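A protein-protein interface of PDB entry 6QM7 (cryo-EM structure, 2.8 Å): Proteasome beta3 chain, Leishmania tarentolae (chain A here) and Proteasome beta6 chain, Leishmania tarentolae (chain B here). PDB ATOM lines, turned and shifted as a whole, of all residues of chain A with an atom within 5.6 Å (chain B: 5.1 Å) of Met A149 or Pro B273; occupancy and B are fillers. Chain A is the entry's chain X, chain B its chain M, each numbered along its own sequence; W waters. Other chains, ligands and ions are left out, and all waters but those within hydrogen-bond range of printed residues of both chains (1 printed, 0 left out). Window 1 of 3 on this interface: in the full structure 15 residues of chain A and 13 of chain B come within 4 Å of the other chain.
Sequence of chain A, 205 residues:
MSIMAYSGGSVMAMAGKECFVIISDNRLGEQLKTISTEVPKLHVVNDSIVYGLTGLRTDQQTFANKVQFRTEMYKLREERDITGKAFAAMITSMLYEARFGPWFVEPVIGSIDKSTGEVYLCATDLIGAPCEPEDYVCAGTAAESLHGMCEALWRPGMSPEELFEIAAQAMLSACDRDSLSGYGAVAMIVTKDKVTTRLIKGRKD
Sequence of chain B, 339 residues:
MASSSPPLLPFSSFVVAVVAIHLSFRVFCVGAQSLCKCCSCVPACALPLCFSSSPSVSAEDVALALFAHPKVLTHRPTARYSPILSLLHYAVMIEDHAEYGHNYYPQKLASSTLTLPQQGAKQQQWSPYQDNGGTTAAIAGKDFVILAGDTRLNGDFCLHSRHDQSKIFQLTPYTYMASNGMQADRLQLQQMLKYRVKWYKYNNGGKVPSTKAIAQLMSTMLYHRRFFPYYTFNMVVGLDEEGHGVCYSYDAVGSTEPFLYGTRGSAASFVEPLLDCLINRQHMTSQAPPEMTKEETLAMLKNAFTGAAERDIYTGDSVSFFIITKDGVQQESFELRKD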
ATOM      1  N   MET A  14      -0.030 -22.075  27.569  1.00  0.00           N
ATOM      2  CA  MET A  14       0.081 -20.610  27.452  1.00  0.00           C
ATOM      3  C   MET A  14       0.407 -20.026  28.804  1.00  0.00           C
ATOM      4  O   MET A  14      -0.282 -20.390  29.756  1.00  0.00           O
ATOM      5  CB  MET A  14      -1.254 -20.035  27.006  1.00  0.00           C
ATOM      6  CG  MET A  14      -1.165 -19.503  25.641  1.00  0.00           C
ATOM      7  SD  MET A  14      -2.714 -18.881  25.088  1.00  0.00           S
ATOM      8  CE  MET A  14      -2.304 -18.671  23.352  1.00  0.00           C
ATOM      9  N   SER A 145      -1.689 -24.359  12.794  1.00  0.00           N
ATOM     10  CA  SER A 145      -2.794 -23.372  12.933  1.00  0.00           C
ATOM     11  C   SER A 145      -2.830 -22.754  14.334  1.00  0.00           C
ATOM     12  O   SER A 145      -3.259 -21.614  14.443  1.00  0.00           O
ATOM     13  CB  SER A 145      -4.118 -23.978  12.561  1.00  0.00           C
ATOM     14  OG  SER A 145      -4.119 -24.375  11.194  1.00  0.00           O
ATOM     15  N   LEU A 146      -2.395 -23.472  15.358  1.00  0.00           N
ATOM     16  CA  LEU A 146      -2.384 -22.993  16.767  1.00  0.00           C
ATOM     17  C   LEU A 146      -1.319 -21.907  16.928  1.00  0.00           C
ATOM     18  O   LEU A 146      -1.638 -20.862  17.512  1.00  0.00           O
ATOM     19  CB  LEU A 146      -2.083 -24.169  17.700  1.00  0.00           C
ATOM     20  CG  LEU A 146      -3.301 -24.943  18.200  1.00  0.00           C
ATOM     21  CD1 LEU A 146      -2.878 -26.280  18.788  1.00  0.00           C
ATOM     22  CD2 LEU A 146      -4.085 -24.121  19.222  1.00  0.00           C
ATOM     23  N   HIS A 147      -0.096 -22.183  16.462  1.00  0.00           N
ATOM     24  CA  HIS A 147       1.032 -21.216  16.387  1.00  0.00           C
ATOM     25  C   HIS A 147       0.543 -19.876  15.830  1.00  0.00           C
ATOM     26  O   HIS A 147       0.956 -18.846  16.362  1.00  0.00           O
ATOM     27  CB  HIS A 147       2.180 -21.763  15.528  1.00  0.00           C
ATOM     28  CG  HIS A 147       3.115 -22.638  16.285  1.00  0.00           C
ATOM     29  ND1 HIS A 147       3.313 -23.970  15.964  1.00  0.00           N
ATOM     30  CD2 HIS A 147       3.900 -22.378  17.350  1.00  0.00           C
ATOM     31  CE1 HIS A 147       4.189 -24.491  16.797  1.00  0.00           C
ATOM     32  NE2 HIS A 147       4.560 -23.536  17.662  1.00  0.00           N
ATOM     33  N   GLY A 148      -0.279 -19.896  14.782  1.00  0.00           N
ATOM     34  CA  GLY A 148      -0.795 -18.671  14.153  1.00  0.00           C
ATOM     35  C   GLY A 148      -1.713 -17.917  15.089  1.00  0.00           C
ATOM     36  O   GLY A 148      -1.586 -16.679  15.184  1.00  0.00           O
ATOM     37  N   MET A 149      -2.618 -18.646  15.736  1.00  0.00           N
ATOM     38  CA  MET A 149      -3.647 -18.095  16.654  1.00  0.00           C
ATOM     39  C   MET A 149      -2.968 -17.561  17.913  1.00  0.00           C
ATOM     40  O   MET A 149      -3.315 -16.461  18.351  1.00  0.00           O
ATOM     41  CB  MET A 149      -4.643 -19.182  17.065  1.00  0.00           C
ATOM     42  CG  MET A 149      -5.594 -19.590  15.967  1.00  0.00           C
ATOM     43  SD  MET A 149      -6.555 -18.193  15.361  1.00  0.00           S
ATOM     44  CE  MET A 149      -7.211 -17.483  16.867  1.00  0.00           C
ATOM     45  N   CYS A 150      -2.054 -18.338  18.482  1.00  0.00           N
ATOM     46  CA  CYS A 150      -1.370 -18.008  19.752  1.00  0.00           C
ATOM     47  C   CYS A 150      -0.434 -16.813  19.525  1.00  0.00           C
ATOM     48  O   CYS A 150      -0.413 -15.934  20.384  1.00  0.00           O
ATOM     49  CB  CYS A 150      -0.650 -19.229  20.306  1.00  0.00           C
ATOM     50  SG  CYS A 150      -1.767 -20.618  20.654  1.00  0.00           S
ATOM     51  N   GLU A 151       0.275 -16.758  18.396  1.00  0.00           N
ATOM     52  CA  GLU A 151       1.180 -15.633  18.029  1.00  0.00           C
ATOM     53  C   GLU A 151       0.399 -14.317  18.008  1.00  0.00           C
ATOM     54  O   GLU A 151       0.940 -13.281  18.487  1.00  0.00           O
ATOM     55  CB  GLU A 151       1.813 -15.858  16.651  1.00  0.00           C
ATOM     56  CG  GLU A 151       2.689 -14.707  16.143  1.00  0.00           C
ATOM     57  CD  GLU A 151       3.864 -14.278  17.019  1.00  0.00           C
ATOM     58  OE1 GLU A 151       4.287 -13.098  16.912  1.00  0.00           O
ATOM     59  OE2 GLU A 151       4.365 -15.125  17.806  1.00  0.00           O
ATOM     60  N   ALA A 152      -0.807 -14.371  17.445  1.00  0.00           N
ATOM     61  CA  ALA A 152      -1.694 -13.215  17.211  1.00  0.00           C
ATOM     62  C   ALA A 152      -2.305 -12.722  18.526  1.00  0.00           C
ATOM     63  O   ALA A 152      -2.201 -11.511  18.803  1.00  0.00           O
ATOM     64  CB  ALA A 152      -2.761 -13.625  16.233  1.00  0.00           C
ATOM     65  N   LEU A 153      -2.917 -13.626  19.297  1.00  0.00           N
ATOM     66  CA  LEU A 153      -3.805 -13.282  20.438  1.00  0.00           C
ATOM     67  C   LEU A 153      -2.997 -13.108  21.727  1.00  0.00           C
ATOM     68  O   LEU A 153      -3.467 -12.358  22.614  1.00  0.00           O
ATOM     69  CB  LEU A 153      -4.854 -14.380  20.647  1.00  0.00           C
ATOM     70  CG  LEU A 153      -5.746 -14.734  19.455  1.00  0.00           C
ATOM     71  CD1 LEU A 153      -6.826 -15.708  19.897  1.00  0.00           C
ATOM     72  CD2 LEU A 153      -6.367 -13.500  18.806  1.00  0.00           C
ATOM     73  N   TRP A 154      -1.869 -13.801  21.860  1.00  0.00           N
ATOM     74  CA  TRP A 154      -1.123 -13.876  23.138  1.00  0.00           C
ATOM     75  C   TRP A 154      -0.357 -12.575  23.384  1.00  0.00           C
ATOM     76  O   TRP A 154       0.313 -12.107  22.439  1.00  0.00           O
ATOM     77  CB  TRP A 154      -0.175 -15.073  23.137  1.00  0.00           C
ATOM     78  CG  TRP A 154       0.487 -15.263  24.460  1.00  0.00           C
ATOM     79  CD1 TRP A 154       0.005 -15.964  25.524  1.00  0.00           C
ATOM     80  CD2 TRP A 154       1.729 -14.682  24.875  1.00  0.00           C
ATOM     81  NE1 TRP A 154       0.874 -15.871  26.573  1.00  0.00           N
ATOM     82  CE2 TRP A 154       1.945 -15.102  26.205  1.00  0.00           C
ATOM     83  CE3 TRP A 154       2.677 -13.859  24.252  1.00  0.00           C
ATOM     84  CZ2 TRP A 154       3.075 -14.718  26.925  1.00  0.00           C
ATOM     85  CZ3 TRP A 154       3.795 -13.478  24.961  1.00  0.00           C
ATOM     86  CH2 TRP A 154       3.993 -13.914  26.278  1.00  0.00           C
ATOM     87  N   GLN A 169     -10.205 -19.491  22.289  1.00  0.00           N
ATOM     88  CA  GLN A 169     -10.372 -18.958  20.906  1.00  0.00           C
ATOM     89  C   GLN A 169      -9.276 -19.476  19.975  1.00  0.00           C
ATOM     90  O   GLN A 169      -9.567 -19.682  18.798  1.00  0.00           O
ATOM     91  CB  GLN A 169     -10.343 -17.429  20.883  1.00  0.00           C
ATOM     92  CG  GLN A 169     -11.571 -16.790  21.514  1.00  0.00           C
ATOM     93  CD  GLN A 169     -12.843 -17.402  20.990  1.00  0.00           C
ATOM     94  OE1 GLN A 169     -13.052 -17.485  19.783  1.00  0.00           O
ATOM     95  NE2 GLN A 169     -13.681 -17.871  21.897  1.00  0.00           N
ATOM     96  N   ALA A 170      -8.056 -19.637  20.468  1.00  0.00           N
ATOM     97  CA  ALA A 170      -6.946 -20.209  19.679  1.00  0.00           C
ATOM     98  C   ALA A 170      -7.254 -21.678  19.417  1.00  0.00           C
ATOM     99  O   ALA A 170      -7.294 -22.054  18.240  1.00  0.00           O
ATOM    100  CB  ALA A 170      -5.617 -20.025  20.364  1.00  0.00           C
ATOM    101  N   MET A 171      -7.482 -22.470  20.462  1.00  0.00           N
ATOM    102  CA  MET A 171      -7.650 -23.934  20.308  1.00  0.00           C
ATOM    103  C   MET A 171      -8.839 -24.188  19.385  1.00  0.00           C
ATOM    104  O   MET A 171      -8.655 -24.968  18.448  1.00  0.00           O
ATOM    105  CB  MET A 171      -7.855 -24.664  21.640  1.00  0.00           C
ATOM    106  CG  MET A 171      -8.057 -26.184  21.501  1.00  0.00           C
ATOM    107  SD  MET A 171      -6.795 -27.073  20.513  1.00  0.00           S
ATOM    108  CE  MET A 171      -5.519 -27.367  21.731  1.00  0.00           C
ATOM    109  N   SER A 173     -10.427 -22.146  17.081  1.00  0.00           N
ATOM    110  CA  SER A 173     -10.246 -21.598  15.718  1.00  0.00           C
ATOM    111  C   SER A 173      -9.266 -22.464  14.930  1.00  0.00           C
ATOM    112  O   SER A 173      -9.521 -22.701  13.733  1.00  0.00           O
ATOM    113  CB  SER A 173      -9.830 -20.164  15.777  1.00  0.00           C
ATOM    114  OG  SER A 173     -10.840 -19.418  16.463  1.00  0.00           O
ATOM    115  N   ALA A 174      -8.218 -22.946  15.587  1.00  0.00           N
ATOM    116  CA  ALA A 174      -7.188 -23.822  14.992  1.00  0.00           C
ATOM    117  C   ALA A 174      -7.761 -25.212  14.700  1.00  0.00           C
ATOM    118  O   ALA A 174      -7.408 -25.804  13.665  1.00  0.00           O
ATOM    119  CB  ALA A 174      -6.017 -23.930  15.932  1.00  0.00           C
ATOM    120  N   ARG A 177     -10.001 -25.622  11.573  1.00  0.00           N
ATOM    121  CA  ARG A 177      -9.226 -25.761  10.320  1.00  0.00           C
ATOM    122  C   ARG A 177      -8.445 -27.077  10.324  1.00  0.00           C
ATOM    123  O   ARG A 177      -7.581 -27.229   9.451  1.00  0.00           O
ATOM    124  CB  ARG A 177      -8.298 -24.555  10.173  1.00  0.00           C
ATOM    125  CG  ARG A 177      -9.016 -23.302   9.709  1.00  0.00           C
ATOM    126  CD  ARG A 177      -9.488 -23.430   8.276  1.00  0.00           C
ATOM    127  NE  ARG A 177     -10.208 -22.235   7.897  1.00  0.00           N
ATOM    128  CZ  ARG A 177     -10.785 -22.031   6.726  1.00  0.00           C
ATOM    129  NH1 ARG A 177     -10.733 -22.949   5.777  1.00  0.00           N
ATOM    130  NH2 ARG A 177     -11.420 -20.895   6.501  1.00  0.00           N
ATOM    131  N   ALA B 268      -0.290 -19.566   5.248  1.00  0.00           N
ATOM    132  CA  ALA B 268      -1.757 -19.552   5.047  1.00  0.00           C
ATOM    133  C   ALA B 268      -2.428 -20.268   6.212  1.00  0.00           C
ATOM    134  O   ALA B 268      -3.468 -19.783   6.673  1.00  0.00           O
ATOM    135  CB  ALA B 268      -2.127 -20.205   3.748  1.00  0.00           C
ATOM    136  N   SER B 269      -1.815 -21.359   6.671  1.00  0.00           N
ATOM    137  CA  SER B 269      -2.285 -22.219   7.784  1.00  0.00           C
ATOM    138  C   SER B 269      -2.267 -21.449   9.117  1.00  0.00           C
ATOM    139  O   SER B 269      -2.980 -21.883  10.025  1.00  0.00           O
ATOM    140  CB  SER B 269      -1.456 -23.490   7.841  1.00  0.00           C
ATOM    141  OG  SER B 269      -2.197 -24.576   8.376  1.00  0.00           O
ATOM    142  N   PHE B 270      -1.479 -20.373   9.247  1.00  0.00           N
ATOM    143  CA  PHE B 270      -1.457 -19.482  10.443  1.00  0.00           C
ATOM    144  C   PHE B 270      -2.524 -18.400  10.335  1.00  0.00           C
ATOM    145  O   PHE B 270      -3.179 -18.058  11.345  1.00  0.00           O
ATOM    146  CB  PHE B 270      -0.185 -18.641  10.588  1.00  0.00           C
ATOM    147  CG  PHE B 270       1.096 -19.403  10.736  1.00  0.00           C
ATOM    148  CD1 PHE B 270       2.280 -18.709  10.833  1.00  0.00           C
ATOM    149  CD2 PHE B 270       1.133 -20.791  10.740  1.00  0.00           C
ATOM    150  CE1 PHE B 270       3.482 -19.389  10.943  1.00  0.00           C
ATOM    151  CE2 PHE B 270       2.335 -21.472  10.850  1.00  0.00           C
ATOM    152  CZ  PHE B 270       3.512 -20.768  10.953  1.00  0.00           C
ATOM    153  N   VAL B 271      -2.620 -17.824   9.148  1.00  0.00           N
ATOM    154  CA  VAL B 271      -3.387 -16.582   8.909  1.00  0.00           C
ATOM    155  C   VAL B 271      -4.869 -16.931   8.767  1.00  0.00           C
ATOM    156  O   VAL B 271      -5.689 -16.165   9.284  1.00  0.00           O
ATOM    157  CB  VAL B 271      -2.805 -15.856   7.691  1.00  0.00           C
ATOM    158  CG1 VAL B 271      -3.666 -14.675   7.257  1.00  0.00           C
ATOM    159  CG2 VAL B 271      -1.373 -15.423   7.960  1.00  0.00           C
ATOM    160  N   GLU B 272      -5.199 -18.053   8.123  1.00  0.00           N
ATOM    161  CA  GLU B 272      -6.600 -18.433   7.795  1.00  0.00           C
ATOM    162  C   GLU B 272      -7.391 -18.667   9.078  1.00  0.00           C
ATOM    163  O   GLU B 272      -8.486 -18.137   9.200  1.00  0.00           O
ATOM    164  CB  GLU B 272      -6.651 -19.644   6.861  1.00  0.00           C
ATOM    165  CG  GLU B 272      -7.998 -19.845   6.176  1.00  0.00           C
ATOM    166  CD  GLU B 272      -7.938 -20.308   4.723  1.00  0.00           C
ATOM    167  OE1 GLU B 272      -7.574 -21.486   4.491  1.00  0.00           O
ATOM    168  OE2 GLU B 272      -8.253 -19.484   3.819  1.00  0.00           O
ATOM    169  N   PRO B 273      -6.894 -19.431  10.077  1.00  0.00           N
ATOM    170  CA  PRO B 273      -7.573 -19.551  11.365  1.00  0.00           C
ATOM    171  C   PRO B 273      -7.781 -18.229  12.102  1.00  0.00           C
ATOM    172  O   PRO B 273      -8.772 -18.102  12.771  1.00  0.00           O
ATOM    173  CB  PRO B 273      -6.620 -20.360  12.239  1.00  0.00           C
ATOM    174  CG  PRO B 273      -5.800 -21.129  11.258  1.00  0.00           C
ATOM    175  CD  PRO B 273      -5.678 -20.242  10.034  1.00  0.00           C
ATOM    176  N   LEU B 274      -6.804 -17.334  12.030  1.00  0.00           N
ATOM    177  CA  LEU B 274      -6.867 -16.004  12.676  1.00  0.00           C
ATOM    178  C   LEU B 274      -7.947 -15.173  11.998  1.00  0.00           C
ATOM    179  O   LEU B 274      -8.638 -14.441  12.708  1.00  0.00           O
ATOM    180  CB  LEU B 274      -5.510 -15.310  12.562  1.00  0.00           C
ATOM    181  CG  LEU B 274      -5.495 -13.874  13.067  1.00  0.00           C
ATOM    182  CD1 LEU B 274      -5.809 -13.843  14.551  1.00  0.00           C
ATOM    183  CD2 LEU B 274      -4.162 -13.208  12.768  1.00  0.00           C
ATOM    184  N   LEU B 275      -8.051 -15.244  10.672  1.00  0.00           N
ATOM    185  CA  LEU B 275      -9.049 -14.457   9.908  1.00  0.00           C
ATOM    186  C   LEU B 275     -10.431 -15.029  10.214  1.00  0.00           C
ATOM    187  O   LEU B 275     -11.314 -14.220  10.508  1.00  0.00           O
ATOM    188  CB  LEU B 275      -8.724 -14.489   8.411  1.00  0.00           C
ATOM    189  CG  LEU B 275      -7.407 -13.828   7.990  1.00  0.00           C
ATOM    190  CD1 LEU B 275      -7.261 -13.807   6.473  1.00  0.00           C
ATOM    191  CD2 LEU B 275      -7.268 -12.420   8.547  1.00  0.00           C
ATOM    192  N   ASP B 276     -10.585 -16.355  10.206  1.00  0.00           N
ATOM    193  CA  ASP B 276     -11.811 -17.064  10.669  1.00  0.00           C
ATOM    194  C   ASP B 276     -12.232 -16.517  12.035  1.00  0.00           C
ATOM    195  O   ASP B 276     -13.421 -16.197  12.184  1.00  0.00           O
ATOM    196  CB  ASP B 276     -11.630 -18.574  10.875  1.00  0.00           C
ATOM    197  CG  ASP B 276     -11.321 -19.412   9.644  1.00  0.00           C
ATOM    198  OD1 ASP B 276     -11.626 -18.971   8.521  1.00  0.00           O
ATOM    199  OD2 ASP B 276     -10.780 -20.523   9.828  1.00  0.00           O
ATOM    200  N   CYS B 277     -11.307 -16.479  12.997  1.00  0.00           N
ATOM    201  CA  CYS B 277     -11.567 -16.068  14.402  1.00  0.00           C
ATOM    202  C   CYS B 277     -12.083 -14.627  14.425  1.00  0.00           C
ATOM    203  O   CYS B 277     -13.147 -14.405  15.012  1.00  0.00           O
ATOM    204  CB  CYS B 277     -10.317 -16.183  15.269  1.00  0.00           C
ATOM    205  SG  CYS B 277     -10.581 -15.852  17.034  1.00  0.00           S
HETATM  206  O   HOH W   1     -13.766 -17.446  17.323  1.00  0.00           O
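The backbone carbonyl oxygen (O) of Ser B269 sits at hydrogen-bond distance from the side-chain hydroxyl (OG) of Ser A145 (3.0 Å). The side-chain sulfur of Met A149 is in hydrogen-bond range of the backbone NH of Leu B274 (3.4 Å). The side-chain hydroxyl (OG) of Ser A173 sits close to the side-chain sulfur (SG) of Cys B277 (3.6 Å). NH1 of Arg A177 lies within salt-bridge range of OE1 of Glu B272, 3.7 Å away. NE of Arg A177 is in salt-bridge range of OD2 of Asp B276 (2.6 Å). SD of Met A149 sits close to O of Pro B273 (3.4 Å).
OG of Ser A173 lies within hydrogen-bond range of O of Gln A169, 2.7 Å away.
Of the 17 printed residues of chain A, 6 touch a printed residue of chain B. Hydrophobic or aromatic side chains of chain A within 4 Å of the printed part of chain B: Met A149 and Ala A152. Of the 10 printed residues of chain B, 7 touch a printed residue of chain A. Among the printed residues, Asp or Glu carboxylates within 4 Å of a Lys or Arg side-chain nitrogen of the other chain: Arg A177 with Glu B272 (3.7 Å) and Arg A177 with Asp B276 (2.6 Å).
Among the printed residues, merely in contact across the chains: Ser A145 with Pro B273 (3.6 Å), Gly A148 with Phe B270 (3.6 Å), Met A149 with Cys B277 (3.7 Å), Ala A152 with Leu B274 (3.5 Å) and Ser A173 with Pro B273 (3.8 Å).
Printed residues of chain B within 4 Å of Gly A148: Phe B270 (3.6 Å). Of chain B, only Pro B273, Leu B274 and Cys B277 come within 4 Å of Met A149. Of the printed residues of chain B, Ala A152 touches Leu B274. Gln A169 touches none of the printed residues of chain B. Of the printed residues of chain B, Ser A173 touches Pro B273 and Cys B277. Ala B268 touches none of the printed residues of chain A. Printed residues of chain A within 4 Å of Ser B269: Ser A145 (3.0 Å). Pro B273 touches just these residues of chain A: Ser A145 (3.6 Å), Met A149 (3.4 Å) and Ser A173 (3.8 Å). Of the printed residues of chain A, Asp B276 touches Arg A177. The nearest residue of chain B that does not touch Met A149 is Phe B270 (4.5 Å).
Water W1 lies within hydrogen-bond range of the side-chain amide oxygen of Gln A169 and the side-chain sulfur of Cys B277.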
